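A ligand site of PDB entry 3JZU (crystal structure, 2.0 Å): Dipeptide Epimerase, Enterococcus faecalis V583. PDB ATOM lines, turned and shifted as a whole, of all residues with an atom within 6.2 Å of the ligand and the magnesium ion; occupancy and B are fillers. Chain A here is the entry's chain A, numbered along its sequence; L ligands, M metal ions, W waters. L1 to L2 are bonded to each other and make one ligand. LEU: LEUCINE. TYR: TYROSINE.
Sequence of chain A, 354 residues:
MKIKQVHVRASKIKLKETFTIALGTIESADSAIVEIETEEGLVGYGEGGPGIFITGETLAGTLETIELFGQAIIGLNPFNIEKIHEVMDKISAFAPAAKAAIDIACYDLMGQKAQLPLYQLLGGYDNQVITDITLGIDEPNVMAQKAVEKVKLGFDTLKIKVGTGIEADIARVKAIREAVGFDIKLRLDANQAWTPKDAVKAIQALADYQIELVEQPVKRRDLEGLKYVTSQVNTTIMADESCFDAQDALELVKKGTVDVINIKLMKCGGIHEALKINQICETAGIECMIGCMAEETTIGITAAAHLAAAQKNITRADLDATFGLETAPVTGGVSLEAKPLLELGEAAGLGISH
OD2 of Asp 318 is in salt-bridge range of N of LEU L1, at 2.6 Å. An oxygen (OH) of TYR L2 is in hydrogen-bond range of the side-chain carboxylate (OE1) of Glu 295 (2.6 Å). O of Cys 292 lies within hydrogen-bond range of N of TYR L2 (2.8 Å). N of LEU L1 is in salt-bridge range of OD1 of Asp 320, at 2.8 Å. The side-chain amide nitrogen (ND2) of Asn 191 sits close to an oxygen (OXT) of TYR L2, 2.9 Å away. NZ of Lys 161 lies within salt-bridge range of O of TYR L2, 3.9 Å away. An oxygen (O) of TYR L2 is in salt-bridge range of the side-chain amino group (NZ) of Lys 159. OG1 of Thr 134 lies within hydrogen-bond range of N of LEU L1 (3.1 Å). An oxygen (O) of TYR L2 is in salt-bridge range of the side-chain amino group (NZ) of Lys 264 (3.5 Å).
The side-chain carboxylate (OE1) of Glu 215 lies within salt-bridge range of the side-chain amino group (NZ) of Lys 159 (2.9 Å). OE2 of Glu 215 sits close to ND2 of Asn 262 (2.8 Å). OD1 of Asp 189 lies within salt-bridge range of NZ of Lys 161 (3.95 Å). NZ of Lys 264 is in salt-bridge range of OD1 of Asp 240 (2.7 Å). OE1 of Gln 216 lies within hydrogen-bond range of N of Asp 240, 2.9 Å away. OD1 of Asn 191 sits at hydrogen-bond distance from NZ of Lys 161, at 2.8 Å. The backbone NH (N) of Phe 19 is in hydrogen-bond range of the backbone carbonyl oxygen (O) of Ile 26 (2.9 Å). NZ of Lys 264 sits at hydrogen-bond distance from OD1 of Asn 262 (2.7 Å).
OE2 of Glu 215 binds the magnesium ion, 2.1 Å away. The magnesium ion is bound by water W1, 2.2 Å away. The side-chain carboxylate (OD2) of Asp 189 binds the magnesium ion, at 2.3 Å. OD2 of Asp 240 binds the magnesium ion, 2.3 Å away. The magnesium ion is bound by an oxygen (OXT) of TYR L2, 2.5 Å away. Slightly farther from the magnesium ion lies an oxygen (O) of TYR L2 (2.6 Å).
Merely in contact with the ligand: Phe 19, Ile 21, Ile 26, Phe 53, Met 293, Ala 294 and Ala 321. Hydrophobic or aromatic side chains within 4 Å of the ligand: Phe 19, Ile 21, Ile 26, Phe 53, Met 293, Ala 294 and Ala 321.
Lys 159 touches the magnesium ion. ND2 of Asn 191 touches the magnesium ion, at 3.98 Å. Five residues have an atom within 4 Å of the magnesium ion: Lys 159, Asp 189, Asn 191, Glu 215 and Asp 240. The nearest printed residue that does not touch the magnesium ion is Lys 161 (4.1 Å).
Water W1 lies within hydrogen-bond range of the side-chain carboxylate (OE1) of Glu 241, the side-chain carboxylate (OD1) of Asp 189 and the side-chain amide nitrogen (ND2) of Asn 191.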
ATOM      1  N   LEU A  15      16.673 -11.725  19.513  1.00  0.00           N
ATOM      2  CA  LEU A  15      17.794 -11.008  18.911  1.00  0.00           C
ATOM      3  C   LEU A  15      18.624 -10.462  20.067  1.00  0.00           C
ATOM      4  O   LEU A  15      18.071 -10.154  21.126  1.00  0.00           O
ATOM      5  CB  LEU A  15      17.313  -9.850  18.026  1.00  0.00           C
ATOM      6  CG  LEU A  15      16.444 -10.217  16.814  1.00  0.00           C
ATOM      7  CD1 LEU A  15      16.258  -8.980  15.942  1.00  0.00           C
ATOM      8  CD2 LEU A  15      17.102 -11.322  16.018  1.00  0.00           C
ATOM      9  N   PHE A  19      16.124  -3.949  17.255  1.00  0.00           N
ATOM     10  CA  PHE A  19      16.583  -3.176  16.120  1.00  0.00           C
ATOM     11  C   PHE A  19      15.516  -2.170  15.741  1.00  0.00           C
ATOM     12  O   PHE A  19      14.369  -2.543  15.507  1.00  0.00           O
ATOM     13  CB  PHE A  19      16.869  -4.084  14.927  1.00  0.00           C
ATOM     14  CG  PHE A  19      18.128  -3.743  14.204  1.00  0.00           C
ATOM     15  CD1 PHE A  19      19.366  -4.114  14.724  1.00  0.00           C
ATOM     16  CD2 PHE A  19      18.096  -3.027  13.011  1.00  0.00           C
ATOM     17  CE1 PHE A  19      20.547  -3.774  14.066  1.00  0.00           C
ATOM     18  CE2 PHE A  19      19.268  -2.678  12.348  1.00  0.00           C
ATOM     19  CZ  PHE A  19      20.494  -3.053  12.880  1.00  0.00           C
ATOM     20  N   ILE A  21      14.122   0.730  13.128  1.00  0.00           N
ATOM     21  CA  ILE A  21      14.178   1.311  11.794  1.00  0.00           C
ATOM     22  C   ILE A  21      13.018   2.297  11.774  1.00  0.00           C
ATOM     23  O   ILE A  21      12.253   2.373  12.742  1.00  0.00           O
ATOM     24  CB  ILE A  21      14.024   0.270  10.665  1.00  0.00           C
ATOM     25  CG1 ILE A  21      12.661  -0.428  10.736  1.00  0.00           C
ATOM     26  CG2 ILE A  21      15.150  -0.775  10.761  1.00  0.00           C
ATOM     27  CD1 ILE A  21      12.374  -1.281   9.525  1.00  0.00           C
ATOM     28  N   LEU A  23      10.230   2.178  10.343  1.00  0.00           N
ATOM     29  CA  LEU A  23       8.940   1.467  10.411  1.00  0.00           C
ATOM     30  C   LEU A  23       8.540   0.902  11.780  1.00  0.00           C
ATOM     31  O   LEU A  23       7.368   0.612  12.014  1.00  0.00           O
ATOM     32  CB  LEU A  23       8.939   0.341   9.395  1.00  0.00           C
ATOM     33  CG  LEU A  23       9.238   0.788   7.955  1.00  0.00           C
ATOM     34  CD1 LEU A  23       9.374  -0.422   7.046  1.00  0.00           C
ATOM     35  CD2 LEU A  23       8.151   1.727   7.469  1.00  0.00           C
ATOM     36  N   THR A  25      10.150  -1.526  15.430  1.00  0.00           N
ATOM     37  CA  THR A  25      11.228  -2.305  16.033  1.00  0.00           C
ATOM     38  C   THR A  25      11.029  -3.781  15.803  1.00  0.00           C
ATOM     39  O   THR A  25       9.923  -4.240  15.494  1.00  0.00           O
ATOM     40  CB  THR A  25      11.283  -2.075  17.543  1.00  0.00           C
ATOM     41  OG1 THR A  25      10.030  -2.477  18.122  1.00  0.00           O
ATOM     42  CG2 THR A  25      11.555  -0.595  17.864  1.00  0.00           C
ATOM     43  N   ILE A  26      12.117  -4.536  15.949  1.00  0.00           N
ATOM     44  CA  ILE A  26      12.083  -5.982  15.806  1.00  0.00           C
ATOM     45  C   ILE A  26      12.966  -6.486  16.948  1.00  0.00           C
ATOM     46  O   ILE A  26      14.056  -5.950  17.191  1.00  0.00           O
ATOM     47  CB  ILE A  26      12.644  -6.416  14.433  1.00  0.00           C
ATOM     48  CG1 ILE A  26      12.248  -7.865  14.125  1.00  0.00           C
ATOM     49  CG2 ILE A  26      14.146  -6.249  14.393  1.00  0.00           C
ATOM     50  CD1 ILE A  26      12.888  -8.898  15.022  1.00  0.00           C
ATOM     51  N   PRO A  50       8.867 -13.835   7.731  1.00  0.00           N
ATOM     52  CA  PRO A  50       8.061 -12.656   7.440  1.00  0.00           C
ATOM     53  C   PRO A  50       8.318 -11.392   8.270  1.00  0.00           C
ATOM     54  O   PRO A  50       8.490 -11.460   9.484  1.00  0.00           O
ATOM     55  CB  PRO A  50       6.643 -13.164   7.629  1.00  0.00           C
ATOM     56  CG  PRO A  50       6.792 -14.021   8.860  1.00  0.00           C
ATOM     57  CD  PRO A  50       8.127 -14.772   8.609  1.00  0.00           C
ATOM     58  N   GLY A  51       8.304 -10.254   7.588  1.00  0.00           N
ATOM     59  CA  GLY A  51       8.481  -8.966   8.251  1.00  0.00           C
ATOM     60  C   GLY A  51       7.127  -8.284   8.152  1.00  0.00           C
ATOM     61  O   GLY A  51       6.772  -7.774   7.084  1.00  0.00           O
ATOM     62  N   ILE A  52       6.386  -8.272   9.256  1.00  0.00           N
ATOM     63  CA  ILE A  52       5.059  -7.697   9.286  1.00  0.00           C
ATOM     64  C   ILE A  52       4.970  -6.235   8.810  1.00  0.00           C
ATOM     65  O   ILE A  52       4.060  -5.899   8.065  1.00  0.00           O
ATOM     66  CB  ILE A  52       4.418  -7.837  10.703  1.00  0.00           C
ATOM     67  CG1 ILE A  52       2.924  -7.509  10.646  1.00  0.00           C
ATOM     68  CG2 ILE A  52       5.143  -6.959  11.712  1.00  0.00           C
ATOM     69  CD1 ILE A  52       2.150  -7.878  11.906  1.00  0.00           C
ATOM     70  N   PHE A  53       5.914  -5.388   9.208  1.00  0.00           N
ATOM     71  CA  PHE A  53       5.799  -4.012   8.740  1.00  0.00           C
ATOM     72  C   PHE A  53       6.348  -3.800   7.332  1.00  0.00           C
ATOM     73  O   PHE A  53       6.509  -2.671   6.884  1.00  0.00           O
ATOM     74  CB  PHE A  53       6.389  -3.010   9.755  1.00  0.00           C
ATOM     75  CG  PHE A  53       7.775  -3.336  10.239  1.00  0.00           C
ATOM     76  CD1 PHE A  53       8.100  -3.135  11.586  1.00  0.00           C
ATOM     77  CD2 PHE A  53       8.767  -3.772   9.373  1.00  0.00           C
ATOM     78  CE1 PHE A  53       9.403  -3.355  12.044  1.00  0.00           C
ATOM     79  CE2 PHE A  53      10.068  -4.002   9.816  1.00  0.00           C
ATOM     80  CZ  PHE A  53      10.383  -3.792  11.159  1.00  0.00           C
ATOM     81  N   ILE A  54       6.603  -4.897   6.629  1.00  0.00           N
ATOM     82  CA  ILE A  54       7.076  -4.810   5.252  1.00  0.00           C
ATOM     83  C   ILE A  54       6.044  -5.436   4.311  1.00  0.00           C
ATOM     84  O   ILE A  54       5.585  -4.801   3.372  1.00  0.00           O
ATOM     85  CB  ILE A  54       8.416  -5.558   5.055  1.00  0.00           C
ATOM     86  CG1 ILE A  54       9.500  -4.902   5.916  1.00  0.00           C
ATOM     87  CG2 ILE A  54       8.826  -5.498   3.586  1.00  0.00           C
ATOM     88  CD1 ILE A  54       9.778  -3.449   5.532  1.00  0.00           C
ATOM     89  N   ASP A 132      27.536  -6.010   4.128  1.00  0.00           N
ATOM     90  CA  ASP A 132      27.693  -4.833   4.965  1.00  0.00           C
ATOM     91  C   ASP A 132      27.053  -5.264   6.275  1.00  0.00           C
ATOM     92  O   ASP A 132      26.714  -6.448   6.455  1.00  0.00           O
ATOM     93  CB  ASP A 132      26.910  -3.632   4.390  1.00  0.00           C
ATOM     94  CG  ASP A 132      25.402  -3.879   4.315  1.00  0.00           C
ATOM     95  OD1 ASP A 132      24.853  -4.620   5.156  1.00  0.00           O
ATOM     96  OD2 ASP A 132      24.745  -3.309   3.408  1.00  0.00           O
ATOM     97  N   THR A 134      24.191  -3.511   9.103  1.00  0.00           N
ATOM     98  CA  THR A 134      23.288  -2.397   9.377  1.00  0.00           C
ATOM     99  C   THR A 134      23.363  -1.920  10.828  1.00  0.00           C
ATOM    100  O   THR A 134      23.462  -2.738  11.746  1.00  0.00           O
ATOM    101  CB  THR A 134      21.828  -2.788   9.081  1.00  0.00           C
ATOM    102  OG1 THR A 134      21.707  -3.204   7.708  1.00  0.00           O
ATOM    103  CG2 THR A 134      20.875  -1.598   9.331  1.00  0.00           C
ATOM    104  N   LYS A 159      25.628   0.074   6.707  1.00  0.00           N
ATOM    105  CA  LYS A 159      24.298   0.494   6.275  1.00  0.00           C
ATOM    106  C   LYS A 159      23.697   1.261   7.438  1.00  0.00           C
ATOM    107  O   LYS A 159      23.467   0.691   8.516  1.00  0.00           O
ATOM    108  CB  LYS A 159      23.433  -0.718   5.909  1.00  0.00           C
ATOM    109  CG  LYS A 159      22.021  -0.358   5.478  1.00  0.00           C
ATOM    110  CD  LYS A 159      21.311  -1.564   4.852  1.00  0.00           C
ATOM    111  CE  LYS A 159      19.858  -1.248   4.537  1.00  0.00           C
ATOM    112  NZ  LYS A 159      19.136  -2.366   3.836  1.00  0.00           N
ATOM    113  N   LYS A 161      20.709   3.293   9.236  1.00  0.00           N
ATOM    114  CA  LYS A 161      19.273   3.477   9.265  1.00  0.00           C
ATOM    115  C   LYS A 161      19.013   4.907   9.694  1.00  0.00           C
ATOM    116  O   LYS A 161      19.668   5.422  10.602  1.00  0.00           O
ATOM    117  CB  LYS A 161      18.634   2.490  10.239  1.00  0.00           C
ATOM    118  CG  LYS A 161      18.628   1.054   9.739  1.00  0.00           C
ATOM    119  CD  LYS A 161      17.668   0.879   8.557  1.00  0.00           C
ATOM    120  CE  LYS A 161      17.727  -0.543   7.999  1.00  0.00           C
ATOM    121  NZ  LYS A 161      16.785  -0.738   6.849  1.00  0.00           N
ATOM    122  N   ASP A 189      19.625   4.153   4.636  1.00  0.00           N
ATOM    123  CA  ASP A 189      18.335   3.515   4.401  1.00  0.00           C
ATOM    124  C   ASP A 189      17.298   4.256   5.237  1.00  0.00           C
ATOM    125  O   ASP A 189      17.315   4.154   6.461  1.00  0.00           O
ATOM    126  CB  ASP A 189      18.349   2.034   4.803  1.00  0.00           C
ATOM    127  CG  ASP A 189      17.090   1.307   4.362  1.00  0.00           C
ATOM    128  OD1 ASP A 189      16.078   1.991   4.080  1.00  0.00           O
ATOM    129  OD2 ASP A 189      17.105   0.054   4.286  1.00  0.00           O
ATOM    130  N   ASN A 191      13.970   3.800   5.023  1.00  0.00           N
ATOM    131  CA  ASN A 191      12.733   3.036   5.134  1.00  0.00           C
ATOM    132  C   ASN A 191      11.475   3.896   4.963  1.00  0.00           C
ATOM    133  O   ASN A 191      10.606   3.902   5.836  1.00  0.00           O
ATOM    134  CB  ASN A 191      12.693   2.237   6.449  1.00  0.00           C
ATOM    135  CG  ASN A 191      13.578   0.992   6.408  1.00  0.00           C
ATOM    136  OD1 ASN A 191      14.582   0.901   7.128  1.00  0.00           O
ATOM    137  ND2 ASN A 191      13.217   0.048   5.548  1.00  0.00           N
ATOM    138  N   GLU A 215      18.796   4.279   0.313  1.00  0.00           N
ATOM    139  CA  GLU A 215      17.766   3.277   0.071  1.00  0.00           C
ATOM    140  C   GLU A 215      16.358   3.766   0.456  1.00  0.00           C
ATOM    141  O   GLU A 215      16.168   4.382   1.505  1.00  0.00           O
ATOM    142  CB  GLU A 215      18.112   2.022   0.870  1.00  0.00           C
ATOM    143  CG  GLU A 215      17.345   0.789   0.480  1.00  0.00           C
ATOM    144  CD  GLU A 215      17.859  -0.449   1.195  1.00  0.00           C
ATOM    145  OE1 GLU A 215      19.010  -0.422   1.697  1.00  0.00           O
ATOM    146  OE2 GLU A 215      17.124  -1.454   1.232  1.00  0.00           O
ATOM    147  N   GLN A 216      15.388   3.500  -0.415  1.00  0.00           N
ATOM    148  CA  GLN A 216      13.978   3.863  -0.240  1.00  0.00           C
ATOM    149  C   GLN A 216      13.720   5.127   0.580  1.00  0.00           C
ATOM    150  O   GLN A 216      13.211   5.060   1.699  1.00  0.00           O
ATOM    151  CB  GLN A 216      13.228   2.673   0.383  1.00  0.00           C
ATOM    152  CG  GLN A 216      11.710   2.692   0.221  1.00  0.00           C
ATOM    153  CD  GLN A 216      11.252   2.625  -1.228  1.00  0.00           C
ATOM    154  OE1 GLN A 216      11.655   1.741  -1.993  1.00  0.00           O
ATOM    155  NE2 GLN A 216      10.411   3.558  -1.609  1.00  0.00           N
ATOM    156  N   ASP A 240      13.579  -0.373  -2.313  1.00  0.00           N
ATOM    157  CA  ASP A 240      13.460  -1.580  -1.509  1.00  0.00           C
ATOM    158  C   ASP A 240      11.987  -1.917  -1.418  1.00  0.00           C
ATOM    159  O   ASP A 240      11.499  -2.755  -2.160  1.00  0.00           O
ATOM    160  CB  ASP A 240      14.053  -1.399  -0.123  1.00  0.00           C
ATOM    161  CG  ASP A 240      13.915  -2.636   0.741  1.00  0.00           C
ATOM    162  OD1 ASP A 240      13.522  -3.708   0.206  1.00  0.00           O
ATOM    163  OD2 ASP A 240      14.205  -2.552   1.956  1.00  0.00           O
ATOM    164  N   GLU A 241      11.270  -1.262  -0.505  1.00  0.00           N
ATOM    165  CA  GLU A 241       9.848  -1.555  -0.368  1.00  0.00           C
ATOM    166  C   GLU A 241       9.074  -1.290  -1.662  1.00  0.00           C
ATOM    167  O   GLU A 241       8.045  -1.924  -1.902  1.00  0.00           O
ATOM    168  CB  GLU A 241       9.228  -0.757   0.790  1.00  0.00           C
ATOM    169  CG  GLU A 241       9.741  -1.172   2.157  1.00  0.00           C
ATOM    170  CD  GLU A 241      10.880  -0.296   2.643  1.00  0.00           C
ATOM    171  OE1 GLU A 241      11.790  -0.004   1.845  1.00  0.00           O
ATOM    172  OE2 GLU A 241      10.858   0.109   3.820  1.00  0.00           O
ATOM    173  N   ASN A 262      16.883  -3.425  -4.384  1.00  0.00           N
ATOM    174  CA  ASN A 262      17.114  -4.346  -3.266  1.00  0.00           C
ATOM    175  C   ASN A 262      16.260  -5.601  -3.452  1.00  0.00           C
ATOM    176  O   ASN A 262      15.033  -5.521  -3.509  1.00  0.00           O
ATOM    177  CB  ASN A 262      16.722  -3.667  -1.940  1.00  0.00           C
ATOM    178  CG  ASN A 262      16.955  -4.560  -0.713  1.00  0.00           C
ATOM    179  OD1 ASN A 262      16.504  -5.707  -0.675  1.00  0.00           O
ATOM    180  ND2 ASN A 262      17.655  -4.030   0.297  1.00  0.00           N
ATOM    181  N   LYS A 264      14.964  -9.273  -2.008  1.00  0.00           N
ATOM    182  CA  LYS A 264      14.815 -10.083  -0.787  1.00  0.00           C
ATOM    183  C   LYS A 264      14.001 -11.314  -1.163  1.00  0.00           C
ATOM    184  O   LYS A 264      12.939 -11.193  -1.779  1.00  0.00           O
ATOM    185  CB  LYS A 264      14.091  -9.320   0.321  1.00  0.00           C
ATOM    186  CG  LYS A 264      14.905  -8.229   0.998  1.00  0.00           C
ATOM    187  CD  LYS A 264      14.148  -7.617   2.149  1.00  0.00           C
ATOM    188  CE  LYS A 264      14.867  -6.399   2.700  1.00  0.00           C
ATOM    189  NZ  LYS A 264      15.056  -5.394   1.627  1.00  0.00           N
ATOM    190  N   MET A 289      21.116  -5.371  -5.123  1.00  0.00           N
ATOM    191  CA  MET A 289      21.729  -5.691  -3.849  1.00  0.00           C
ATOM    192  C   MET A 289      20.833  -6.744  -3.234  1.00  0.00           C
ATOM    193  O   MET A 289      19.605  -6.623  -3.276  1.00  0.00           O
ATOM    194  CB  MET A 289      21.782  -4.481  -2.916  1.00  0.00           C
ATOM    195  CG  MET A 289      22.273  -4.853  -1.505  1.00  0.00           C
ATOM    196  SD  MET A 289      22.512  -3.422  -0.411  1.00  0.00           S
ATOM    197  CE  MET A 289      20.944  -3.290   0.373  1.00  0.00           C
ATOM    198  N   GLY A 291      19.238  -8.451  -0.086  1.00  0.00           N
ATOM    199  CA  GLY A 291      18.968  -8.027   1.278  1.00  0.00           C
ATOM    200  C   GLY A 291      18.288  -9.098   2.112  1.00  0.00           C
ATOM    201  O   GLY A 291      18.250 -10.254   1.711  1.00  0.00           O
ATOM    202  N   CYS A 292      17.757  -8.709   3.261  1.00  0.00           N
ATOM    203  CA  CYS A 292      17.093  -9.689   4.135  1.00  0.00           C
ATOM    204  C   CYS A 292      16.200  -9.051   5.190  1.00  0.00           C
ATOM    205  O   CYS A 292      16.281  -7.854   5.483  1.00  0.00           O
ATOM    206  CB  CYS A 292      18.147 -10.540   4.850  1.00  0.00           C
ATOM    207  SG  CYS A 292      19.184  -9.597   5.994  1.00  0.00           S
ATOM    208  N   MET A 293      15.348  -9.894   5.770  1.00  0.00           N
ATOM    209  CA  MET A 293      14.452  -9.487   6.841  1.00  0.00           C
ATOM    210  C   MET A 293      15.222  -9.830   8.118  1.00  0.00           C
ATOM    211  O   MET A 293      16.052 -10.725   8.109  1.00  0.00           O
ATOM    212  CB  MET A 293      13.160 -10.306   6.793  1.00  0.00           C
ATOM    213  CG  MET A 293      12.383 -10.148   5.505  1.00  0.00           C
ATOM    214  SD  MET A 293      11.923  -8.430   5.227  1.00  0.00           S
ATOM    215  CE  MET A 293      10.715  -8.617   3.889  1.00  0.00           C
ATOM    216  N   ALA A 294      14.953  -9.118   9.212  1.00  0.00           N
ATOM    217  CA  ALA A 294      15.639  -9.408  10.467  1.00  0.00           C
ATOM    218  C   ALA A 294      15.153 -10.754  11.025  1.00  0.00           C
ATOM    219  O   ALA A 294      15.863 -11.412  11.786  1.00  0.00           O
ATOM    220  CB  ALA A 294      15.372  -8.293  11.488  1.00  0.00           C
ATOM    221  N   GLU A 295      13.956 -11.158  10.607  1.00  0.00           N
ATOM    222  CA  GLU A 295      13.349 -12.409  11.069  1.00  0.00           C
ATOM    223  C   GLU A 295      13.905 -13.697  10.444  1.00  0.00           C
ATOM    224  O   GLU A 295      13.490 -14.800  10.795  1.00  0.00           O
ATOM    225  CB  GLU A 295      11.830 -12.354  10.832  1.00  0.00           C
ATOM    226  CG  GLU A 295      11.107 -11.286  11.644  1.00  0.00           C
ATOM    227  CD  GLU A 295      11.075  -9.925  10.972  1.00  0.00           C
ATOM    228  OE1 GLU A 295      11.893  -9.673  10.054  1.00  0.00           O
ATOM    229  OE2 GLU A 295      10.229  -9.097  11.368  1.00  0.00           O
ATOM    230  N   ASP A 318      23.556  -7.207   1.735  1.00  0.00           N
ATOM    231  CA  ASP A 318      23.158  -6.757   3.067  1.00  0.00           C
ATOM    232  C   ASP A 318      22.499  -7.989   3.682  1.00  0.00           C
ATOM    233  O   ASP A 318      21.266  -8.083   3.773  1.00  0.00           O
ATOM    234  CB  ASP A 318      22.161  -5.596   2.944  1.00  0.00           C
ATOM    235  CG  ASP A 318      21.594  -5.155   4.298  1.00  0.00           C
ATOM    236  OD1 ASP A 318      22.379  -4.984   5.242  1.00  0.00           O
ATOM    237  OD2 ASP A 318      20.359  -4.975   4.401  1.00  0.00           O
ATOM    238  N   LEU A 319      23.332  -8.956   4.076  1.00  0.00           N
ATOM    239  CA  LEU A 319      22.877 -10.213   4.680  1.00  0.00           C
ATOM    240  C   LEU A 319      23.490 -10.298   6.073  1.00  0.00           C
ATOM    241  O   LEU A 319      24.476 -11.020   6.293  1.00  0.00           O
ATOM    242  CB  LEU A 319      23.351 -11.386   3.822  1.00  0.00           C
ATOM    243  CG  LEU A 319      22.897 -11.292   2.365  1.00  0.00           C
ATOM    244  CD1 LEU A 319      23.474 -12.426   1.526  1.00  0.00           C
ATOM    245  CD2 LEU A 319      21.371 -11.306   2.336  1.00  0.00           C
ATOM    246  N   ASP A 320      22.873  -9.575   7.005  1.00  0.00           N
ATOM    247  CA  ASP A 320      23.354  -9.494   8.375  1.00  0.00           C
ATOM    248  C   ASP A 320      22.349  -9.983   9.424  1.00  0.00           C
ATOM    249  O   ASP A 320      22.527  -9.725  10.613  1.00  0.00           O
ATOM    250  CB  ASP A 320      23.759  -8.037   8.661  1.00  0.00           C
ATOM    251  CG  ASP A 320      22.652  -7.030   8.359  1.00  0.00           C
ATOM    252  OD1 ASP A 320      21.648  -7.412   7.719  1.00  0.00           O
ATOM    253  OD2 ASP A 320      22.792  -5.844   8.742  1.00  0.00           O
ATOM    254  N   ALA A 321      21.313 -10.688   9.006  1.00  0.00           N
ATOM    255  CA  ALA A 321      20.338 -11.169   9.973  1.00  0.00           C
ATOM    256  C   ALA A 321      20.919 -12.133  11.010  1.00  0.00           C
ATOM    257  O   ALA A 321      20.522 -12.092  12.182  1.00  0.00           O
ATOM    258  CB  ALA A 321      19.153 -11.814   9.266  1.00  0.00           C
ATOM    259  N   THR A 322      21.848 -12.998  10.611  1.00  0.00           N
ATOM    260  CA  THR A 322      22.413 -13.965  11.553  1.00  0.00           C
ATOM    261  C   THR A 322      23.274 -13.344  12.628  1.00  0.00           C
ATOM    262  O   THR A 322      23.414 -13.918  13.722  1.00  0.00           O
ATOM    263  CB  THR A 322      23.277 -15.066  10.854  1.00  0.00           C
ATOM    264  OG1 THR A 322      24.423 -14.466  10.246  1.00  0.00           O
ATOM    265  CG2 THR A 322      22.459 -15.814   9.819  1.00  0.00           C
HETATM  266  N   LEU L   1      19.744  -5.458   6.896  1.00  0.00           N
HETATM  267  CA  LEU L   1      18.366  -5.735   7.401  1.00  0.00           C
HETATM  268  C   LEU L   1      17.355  -4.724   6.864  1.00  0.00           C
HETATM  269  O   LEU L   1      17.644  -3.521   6.815  1.00  0.00           O
HETATM  270  CB  LEU L   1      18.342  -5.680   8.935  1.00  0.00           C
HETATM  271  CG  LEU L   1      19.257  -6.616   9.736  1.00  0.00           C
HETATM  272  CD1 LEU L   1      19.022  -6.415  11.218  1.00  0.00           C
HETATM  273  CD2 LEU L   1      18.966  -8.060   9.356  1.00  0.00           C
HETATM  274  N   TYR L   2      16.174  -5.201   6.481  1.00  0.00           N
HETATM  275  CA  TYR L   2      15.095  -4.351   5.992  1.00  0.00           C
HETATM  276  C   TYR L   2      15.556  -3.267   5.016  1.00  0.00           C
HETATM  277  O   TYR L   2      16.451  -3.549   4.200  1.00  0.00           O
HETATM  278  CB  TYR L   2      14.377  -3.682   7.175  1.00  0.00           C
HETATM  279  CG  TYR L   2      13.780  -4.656   8.176  1.00  0.00           C
HETATM  280  CD1 TYR L   2      13.903  -4.420   9.548  1.00  0.00           C
HETATM  281  CD2 TYR L   2      13.058  -5.777   7.770  1.00  0.00           C
HETATM  282  CE1 TYR L   2      13.330  -5.286  10.482  1.00  0.00           C
HETATM  283  CE2 TYR L   2      12.476  -6.647   8.694  1.00  0.00           C
HETATM  284  CZ  TYR L   2      12.616  -6.387  10.060  1.00  0.00           C
HETATM  285  OH  TYR L   2      12.041  -7.223  10.995  1.00  0.00           O
HETATM  286  OXT TYR L   2      14.997  -2.137   5.089  1.00  0.00           O
HETATM  287 MG    MG M   1      15.881  -1.323   2.926  1.00  0.00          MG
HETATM  288  O   HOH W   1      14.404   0.304   2.612  1.00  0.00           O
HETATM  289  O   HOH W   2      19.639  -8.393  14.033  1.00  0.00           O
HETATM  290  O   HOH W   3      18.145  -5.742   3.145  1.00  0.00           O
